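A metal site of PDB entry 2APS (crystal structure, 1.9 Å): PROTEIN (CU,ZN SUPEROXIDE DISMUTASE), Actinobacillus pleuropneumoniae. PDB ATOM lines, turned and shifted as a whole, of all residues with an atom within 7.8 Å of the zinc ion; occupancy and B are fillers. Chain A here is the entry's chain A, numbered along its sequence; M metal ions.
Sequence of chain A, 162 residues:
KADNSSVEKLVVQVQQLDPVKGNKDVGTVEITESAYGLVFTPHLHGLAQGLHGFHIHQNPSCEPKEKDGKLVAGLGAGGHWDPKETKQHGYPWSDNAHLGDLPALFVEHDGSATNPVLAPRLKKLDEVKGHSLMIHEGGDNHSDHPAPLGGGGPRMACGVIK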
ATOM      1  N   PHE A  54      23.383 -15.022   5.082  1.00  0.00           N
ATOM      2  CA  PHE A  54      23.920 -14.893   3.735  1.00  0.00           C
ATOM      3  C   PHE A  54      22.730 -14.755   2.796  1.00  0.00           C
ATOM      4  O   PHE A  54      21.932 -15.693   2.663  1.00  0.00           O
ATOM      5  CB  PHE A  54      24.719 -16.180   3.427  1.00  0.00           C
ATOM      6  CG  PHE A  54      25.627 -16.105   2.228  1.00  0.00           C
ATOM      7  CD1 PHE A  54      26.364 -14.961   1.945  1.00  0.00           C
ATOM      8  CD2 PHE A  54      25.793 -17.222   1.399  1.00  0.00           C
ATOM      9  CE1 PHE A  54      27.261 -14.931   0.868  1.00  0.00           C
ATOM     10  CE2 PHE A  54      26.676 -17.201   0.333  1.00  0.00           C
ATOM     11  CZ  PHE A  54      27.416 -16.054   0.058  1.00  0.00           C
ATOM     12  N   HIS A  55      22.542 -13.579   2.199  1.00  0.00           N
ATOM     13  CA  HIS A  55      21.406 -13.361   1.294  1.00  0.00           C
ATOM     14  C   HIS A  55      21.741 -12.430   0.140  1.00  0.00           C
ATOM     15  O   HIS A  55      22.678 -11.642   0.210  1.00  0.00           O
ATOM     16  CB  HIS A  55      20.215 -12.716   2.025  1.00  0.00           C
ATOM     17  CG  HIS A  55      20.120 -13.048   3.480  1.00  0.00           C
ATOM     18  ND1 HIS A  55      20.518 -12.167   4.464  1.00  0.00           N
ATOM     19  CD2 HIS A  55      19.614 -14.126   4.122  1.00  0.00           C
ATOM     20  CE1 HIS A  55      20.249 -12.682   5.650  1.00  0.00           C
ATOM     21  NE2 HIS A  55      19.705 -13.871   5.467  1.00  0.00           N
ATOM     22  N   ILE A  56      20.939 -12.513  -0.910  1.00  0.00           N
ATOM     23  CA  ILE A  56      21.104 -11.660  -2.084  1.00  0.00           C
ATOM     24  C   ILE A  56      20.094 -10.529  -1.870  1.00  0.00           C
ATOM     25  O   ILE A  56      18.974 -10.777  -1.429  1.00  0.00           O
ATOM     26  CB  ILE A  56      20.770 -12.397  -3.400  1.00  0.00           C
ATOM     27  CG1 ILE A  56      21.794 -13.514  -3.662  1.00  0.00           C
ATOM     28  CG2 ILE A  56      20.753 -11.446  -4.587  1.00  0.00           C
ATOM     29  CD1 ILE A  56      21.461 -14.358  -4.876  1.00  0.00           C
ATOM     30  N   HIS A  57      20.513  -9.292  -2.105  1.00  0.00           N
ATOM     31  CA  HIS A  57      19.632  -8.150  -1.953  1.00  0.00           C
ATOM     32  C   HIS A  57      19.235  -7.536  -3.293  1.00  0.00           C
ATOM     33  O   HIS A  57      19.796  -7.878  -4.332  1.00  0.00           O
ATOM     34  CB  HIS A  57      20.266  -7.103  -1.031  1.00  0.00           C
ATOM     35  CG  HIS A  57      20.240  -7.486   0.416  1.00  0.00           C
ATOM     36  ND1 HIS A  57      19.649  -6.712   1.381  1.00  0.00           N
ATOM     37  CD2 HIS A  57      20.731  -8.575   1.053  1.00  0.00           C
ATOM     38  CE1 HIS A  57      19.761  -7.310   2.562  1.00  0.00           C
ATOM     39  NE2 HIS A  57      20.424  -8.441   2.384  1.00  0.00           N
ATOM     40  N   GLY A  79      16.295  -4.202   0.402  1.00  0.00           N
ATOM     41  CA  GLY A  79      15.846  -5.372   1.120  1.00  0.00           C
ATOM     42  C   GLY A  79      16.347  -6.628   0.426  1.00  0.00           C
ATOM     43  O   GLY A  79      17.136  -6.563  -0.514  1.00  0.00           O
ATOM     44  N   HIS A  80      15.890  -7.785   0.903  1.00  0.00           N
ATOM     45  CA  HIS A  80      16.280  -9.055   0.314  1.00  0.00           C
ATOM     46  C   HIS A  80      15.688  -9.129  -1.084  1.00  0.00           C
ATOM     47  O   HIS A  80      14.623  -8.552  -1.340  1.00  0.00           O
ATOM     48  CB  HIS A  80      15.783 -10.229   1.180  1.00  0.00           C
ATOM     49  CG  HIS A  80      16.472 -10.356   2.508  1.00  0.00           C
ATOM     50  ND1 HIS A  80      16.296 -11.447   3.338  1.00  0.00           N
ATOM     51  CD2 HIS A  80      17.352  -9.546   3.140  1.00  0.00           C
ATOM     52  CE1 HIS A  80      17.028 -11.279   4.427  1.00  0.00           C
ATOM     53  NE2 HIS A  80      17.674 -10.140   4.330  1.00  0.00           N
ATOM     54  N   TRP A  81      16.371  -9.791  -2.009  1.00  0.00           N
ATOM     55  CA  TRP A  81      15.883  -9.940  -3.367  1.00  0.00           C
ATOM     56  C   TRP A  81      14.661 -10.853  -3.310  1.00  0.00           C
ATOM     57  O   TRP A  81      14.756 -11.989  -2.831  1.00  0.00           O
ATOM     58  CB  TRP A  81      16.985 -10.525  -4.252  1.00  0.00           C
ATOM     59  CG  TRP A  81      16.605 -10.771  -5.667  1.00  0.00           C
ATOM     60  CD1 TRP A  81      15.823  -9.986  -6.459  1.00  0.00           C
ATOM     61  CD2 TRP A  81      16.972 -11.898  -6.454  1.00  0.00           C
ATOM     62  NE1 TRP A  81      15.667 -10.558  -7.698  1.00  0.00           N
ATOM     63  CE2 TRP A  81      16.370 -11.738  -7.723  1.00  0.00           C
ATOM     64  CE3 TRP A  81      17.757 -13.039  -6.220  1.00  0.00           C
ATOM     65  CZ2 TRP A  81      16.528 -12.672  -8.750  1.00  0.00           C
ATOM     66  CZ3 TRP A  81      17.912 -13.962  -7.241  1.00  0.00           C
ATOM     67  CH2 TRP A  81      17.290 -13.775  -8.494  1.00  0.00           C
ATOM     68  N   ASP A  82      13.511 -10.355  -3.766  1.00  0.00           N
ATOM     69  CA  ASP A  82      12.242 -11.095  -3.712  1.00  0.00           C
ATOM     70  C   ASP A  82      11.384 -10.910  -4.989  1.00  0.00           C
ATOM     71  O   ASP A  82      10.248 -10.432  -4.921  1.00  0.00           O
ATOM     72  CB  ASP A  82      11.453 -10.626  -2.462  1.00  0.00           C
ATOM     73  CG  ASP A  82      10.184 -11.443  -2.179  1.00  0.00           C
ATOM     74  OD1 ASP A  82      10.055 -12.582  -2.695  1.00  0.00           O
ATOM     75  OD2 ASP A  82       9.322 -10.955  -1.420  1.00  0.00           O
ATOM     76  N   THR A  86       7.038 -13.122  -2.183  1.00  0.00           N
ATOM     77  CA  THR A  86       6.527 -14.018  -1.152  1.00  0.00           C
ATOM     78  C   THR A  86       6.266 -13.202   0.115  1.00  0.00           C
ATOM     79  O   THR A  86       5.442 -13.583   0.961  1.00  0.00           O
ATOM     80  CB  THR A  86       7.537 -15.120  -0.815  1.00  0.00           C
ATOM     81  OG1 THR A  86       8.718 -14.528  -0.255  1.00  0.00           O
ATOM     82  CG2 THR A  86       7.917 -15.904  -2.079  1.00  0.00           C
ATOM     83  N   GLN A  88       8.028 -12.952   2.624  1.00  0.00           N
ATOM     84  CA  GLN A  88       8.503 -13.613   3.832  1.00  0.00           C
ATOM     85  C   GLN A  88       9.900 -14.239   3.682  1.00  0.00           C
ATOM     86  O   GLN A  88      10.308 -14.666   2.598  1.00  0.00           O
ATOM     87  CB  GLN A  88       7.496 -14.645   4.350  1.00  0.00           C
ATOM     88  CG  GLN A  88       7.207 -15.794   3.411  1.00  0.00           C
ATOM     89  CD  GLN A  88       6.487 -16.929   4.108  1.00  0.00           C
ATOM     90  OE1 GLN A  88       5.274 -17.079   3.965  1.00  0.00           O
ATOM     91  NE2 GLN A  88       7.228 -17.748   4.848  1.00  0.00           N
ATOM     92  N   HIS A  89      10.645 -14.194   4.771  1.00  0.00           N
ATOM     93  CA  HIS A  89      11.984 -14.742   4.812  1.00  0.00           C
ATOM     94  C   HIS A  89      11.844 -16.209   5.213  1.00  0.00           C
ATOM     95  O   HIS A  89      11.009 -16.533   6.058  1.00  0.00           O
ATOM     96  CB  HIS A  89      12.811 -13.996   5.849  1.00  0.00           C
ATOM     97  CG  HIS A  89      14.229 -14.446   5.918  1.00  0.00           C
ATOM     98  ND1 HIS A  89      15.134 -14.152   4.924  1.00  0.00           N
ATOM     99  CD2 HIS A  89      14.890 -15.181   6.842  1.00  0.00           C
ATOM    100  CE1 HIS A  89      16.307 -14.694   5.231  1.00  0.00           C
ATOM    101  NE2 HIS A  89      16.176 -15.327   6.385  1.00  0.00           N
ATOM    102  N   GLY A  90      12.652 -17.070   4.621  1.00  0.00           N
ATOM    103  CA  GLY A  90      12.571 -18.482   4.939  1.00  0.00           C
ATOM    104  C   GLY A  90      13.771 -19.305   4.534  1.00  0.00           C
ATOM    105  O   GLY A  90      14.881 -18.786   4.378  1.00  0.00           O
ATOM    106  N   TYR A  91      13.543 -20.599   4.368  1.00  0.00           N
ATOM    107  CA  TYR A  91      14.572 -21.557   3.986  1.00  0.00           C
ATOM    108  C   TYR A  91      14.984 -21.478   2.531  1.00  0.00           C
ATOM    109  O   TYR A  91      14.172 -21.171   1.658  1.00  0.00           O
ATOM    110  CB  TYR A  91      14.103 -22.974   4.298  1.00  0.00           C
ATOM    111  CG  TYR A  91      13.836 -23.183   5.760  1.00  0.00           C
ATOM    112  CD1 TYR A  91      14.884 -23.467   6.634  1.00  0.00           C
ATOM    113  CD2 TYR A  91      12.549 -23.066   6.268  1.00  0.00           C
ATOM    114  CE1 TYR A  91      14.650 -23.608   7.990  1.00  0.00           C
ATOM    115  CE2 TYR A  91      12.308 -23.211   7.629  1.00  0.00           C
ATOM    116  CZ  TYR A  91      13.361 -23.483   8.483  1.00  0.00           C
ATOM    117  OH  TYR A  91      13.119 -23.621   9.829  1.00  0.00           O
ATOM    118  N   ALA A  97       9.939 -18.766   0.563  1.00  0.00           N
ATOM    119  CA  ALA A  97      11.011 -17.836   0.926  1.00  0.00           C
ATOM    120  C   ALA A  97      11.459 -16.878  -0.176  1.00  0.00           C
ATOM    121  O   ALA A  97      11.143 -17.079  -1.354  1.00  0.00           O
ATOM    122  CB  ALA A  97      12.206 -18.617   1.420  1.00  0.00           C
ATOM    123  N   HIS A  98      12.146 -15.809   0.221  1.00  0.00           N
ATOM    124  CA  HIS A  98      12.672 -14.846  -0.745  1.00  0.00           C
ATOM    125  C   HIS A  98      13.635 -15.637  -1.627  1.00  0.00           C
ATOM    126  O   HIS A  98      14.396 -16.455  -1.118  1.00  0.00           O
ATOM    127  CB  HIS A  98      13.488 -13.742  -0.044  1.00  0.00           C
ATOM    128  CG  HIS A  98      12.721 -12.931   0.962  1.00  0.00           C
ATOM    129  ND1 HIS A  98      13.212 -12.647   2.213  1.00  0.00           N
ATOM    130  CD2 HIS A  98      11.511 -12.326   0.882  1.00  0.00           C
ATOM    131  CE1 HIS A  98      12.335 -11.894   2.863  1.00  0.00           C
ATOM    132  NE2 HIS A  98      11.291 -11.692   2.076  1.00  0.00           N
ATOM    133  N   LEU A  99      13.641 -15.365  -2.927  1.00  0.00           N
ATOM    134  CA  LEU A  99      14.525 -16.082  -3.833  1.00  0.00           C
ATOM    135  C   LEU A  99      16.000 -15.848  -3.469  1.00  0.00           C
ATOM    136  O   LEU A  99      16.849 -16.691  -3.743  1.00  0.00           O
ATOM    137  CB  LEU A  99      14.261 -15.673  -5.276  1.00  0.00           C
ATOM    138  CG  LEU A  99      14.850 -16.538  -6.393  1.00  0.00           C
ATOM    139  CD1 LEU A  99      14.308 -17.968  -6.322  1.00  0.00           C
ATOM    140  CD2 LEU A  99      14.523 -15.905  -7.732  1.00  0.00           C
ATOM    141  N   GLY A 100      16.295 -14.721  -2.803  1.00  0.00           N
ATOM    142  CA  GLY A 100      17.664 -14.411  -2.419  1.00  0.00           C
ATOM    143  C   GLY A 100      18.145 -15.017  -1.111  1.00  0.00           C
ATOM    144  O   GLY A 100      19.261 -14.714  -0.660  1.00  0.00           O
ATOM    145  N   ASP A 101      17.328 -15.838  -0.474  1.00  0.00           N
ATOM    146  CA  ASP A 101      17.690 -16.472   0.795  1.00  0.00           C
ATOM    147  C   ASP A 101      18.614 -17.660   0.581  1.00  0.00           C
ATOM    148  O   ASP A 101      18.171 -18.706   0.100  1.00  0.00           O
ATOM    149  CB  ASP A 101      16.434 -16.911   1.560  1.00  0.00           C
ATOM    150  CG  ASP A 101      15.592 -15.742   2.015  1.00  0.00           C
ATOM    151  OD1 ASP A 101      16.080 -14.584   1.986  1.00  0.00           O
ATOM    152  OD2 ASP A 101      14.422 -15.975   2.418  1.00  0.00           O
ATOM    153  N   LEU A 102      19.876 -17.504   0.964  1.00  0.00           N
ATOM    154  CA  LEU A 102      20.891 -18.548   0.821  1.00  0.00           C
ATOM    155  C   LEU A 102      21.203 -19.219   2.161  1.00  0.00           C
ATOM    156  O   LEU A 102      20.789 -18.736   3.229  1.00  0.00           O
ATOM    157  CB  LEU A 102      22.181 -17.936   0.272  1.00  0.00           C
ATOM    158  CG  LEU A 102      22.022 -16.916  -0.855  1.00  0.00           C
ATOM    159  CD1 LEU A 102      23.342 -16.242  -1.139  1.00  0.00           C
ATOM    160  CD2 LEU A 102      21.463 -17.609  -2.093  1.00  0.00           C
ATOM    161  N   ASP A 140      21.018 -16.696  11.115  1.00  0.00           N
ATOM    162  CA  ASP A 140      19.814 -16.775  10.307  1.00  0.00           C
ATOM    163  C   ASP A 140      19.047 -18.019  10.712  1.00  0.00           C
ATOM    164  O   ASP A 140      19.509 -19.141  10.492  1.00  0.00           O
ATOM    165  CB  ASP A 140      20.232 -16.892   8.834  1.00  0.00           C
ATOM    166  CG  ASP A 140      19.079 -16.681   7.856  1.00  0.00           C
ATOM    167  OD1 ASP A 140      17.903 -16.704   8.270  1.00  0.00           O
ATOM    168  OD2 ASP A 140      19.356 -16.477   6.665  1.00  0.00           O
ATOM    169  N   HIS A 142      16.166 -18.537   9.491  1.00  0.00           N
ATOM    170  CA  HIS A 142      15.293 -18.681   8.320  1.00  0.00           C
ATOM    171  C   HIS A 142      13.801 -18.449   8.579  1.00  0.00           C
ATOM    172  O   HIS A 142      12.951 -19.169   8.056  1.00  0.00           O
ATOM    173  CB  HIS A 142      15.521 -20.037   7.654  1.00  0.00           C
ATOM    174  CG  HIS A 142      16.877 -20.186   7.056  1.00  0.00           C
ATOM    175  ND1 HIS A 142      17.858 -20.986   7.599  1.00  0.00           N
ATOM    176  CD2 HIS A 142      17.440 -19.589   5.974  1.00  0.00           C
ATOM    177  CE1 HIS A 142      18.968 -20.876   6.891  1.00  0.00           C
ATOM    178  NE2 HIS A 142      18.745 -20.034   5.903  1.00  0.00           N
ATOM    179  N   SER A 143      13.500 -17.407   9.340  1.00  0.00           N
ATOM    180  CA  SER A 143      12.124 -17.060   9.677  1.00  0.00           C
ATOM    181  C   SER A 143      12.104 -15.572   9.967  1.00  0.00           C
ATOM    182  O   SER A 143      13.164 -14.965  10.125  1.00  0.00           O
ATOM    183  CB  SER A 143      11.673 -17.830  10.917  1.00  0.00           C
ATOM    184  OG  SER A 143      10.393 -17.404  11.368  1.00  0.00           O
ATOM    185  N   ASP A 144      10.913 -14.980   9.983  1.00  0.00           N
ATOM    186  CA  ASP A 144      10.783 -13.559  10.311  1.00  0.00           C
ATOM    187  C   ASP A 144      10.447 -13.422  11.804  1.00  0.00           C
ATOM    188  O   ASP A 144      10.094 -12.346  12.281  1.00  0.00           O
ATOM    189  CB  ASP A 144       9.676 -12.904   9.486  1.00  0.00           C
ATOM    190  CG  ASP A 144      10.076 -12.669   8.059  1.00  0.00           C
ATOM    191  OD1 ASP A 144      11.110 -12.006   7.831  1.00  0.00           O
ATOM    192  OD2 ASP A 144       9.347 -13.130   7.158  1.00  0.00           O
ATOM    193  N   LEU A 149      13.591 -11.026   9.112  1.00  0.00           N
ATOM    194  CA  LEU A 149      14.651 -11.467   8.202  1.00  0.00           C
ATOM    195  C   LEU A 149      15.701 -12.421   8.801  1.00  0.00           C
ATOM    196  O   LEU A 149      16.894 -12.280   8.544  1.00  0.00           O
ATOM    197  CB  LEU A 149      15.351 -10.260   7.544  1.00  0.00           C
ATOM    198  CG  LEU A 149      14.636  -9.305   6.571  1.00  0.00           C
ATOM    199  CD1 LEU A 149      13.696 -10.049   5.654  1.00  0.00           C
ATOM    200  CD2 LEU A 149      13.877  -8.245   7.326  1.00  0.00           C
ATOM    201  N   GLY A 150      15.255 -13.386   9.599  1.00  0.00           N
ATOM    202  CA  GLY A 150      16.166 -14.370  10.167  1.00  0.00           C
ATOM    203  C   GLY A 150      17.068 -13.907  11.303  1.00  0.00           C
ATOM    204  O   GLY A 150      17.835 -14.716  11.829  1.00  0.00           O
HETATM  205 ZN    ZN M   1      15.117 -13.193   3.062  1.00  0.00          ZN
HETATM  206 CU    CU M   2      20.597  -9.906   4.069  1.00  0.00          CU
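Four residues have an atom within 4 Å of the zinc ion: His 80, His 89, His 98 and Asp 101.
NE2 of His 89 lies within hydrogen-bond range of OD1 of Asp 140 (2.9 Å). NE2 of His 80 sits close to ND1 of His 55 (3.5 Å). The side-chain carboxylate (OD2) of Asp 144 lies within hydrogen-bond range of the backbone NH (N) of His 89 (2.9 Å). The side-chain carboxylate (OD2) of Asp 101 is in hydrogen-bond range of the backbone NH (N) of Gly 90 (3.0 Å). The backbone carbonyl oxygen (O) of Gln 88 sits close to a ring nitrogen (NE2) of His 98.
The zinc ion is bound by OD1 of Asp 101. A ring nitrogen (ND1) of His 89 binds the zinc ion, at 2.1 Å. ND1 of His 80 is bound to the zinc ion. The zinc ion is bound by a ring nitrogen (ND1) of His 98 (2.2 Å). The zinc ion has four donor atoms within binding distance.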
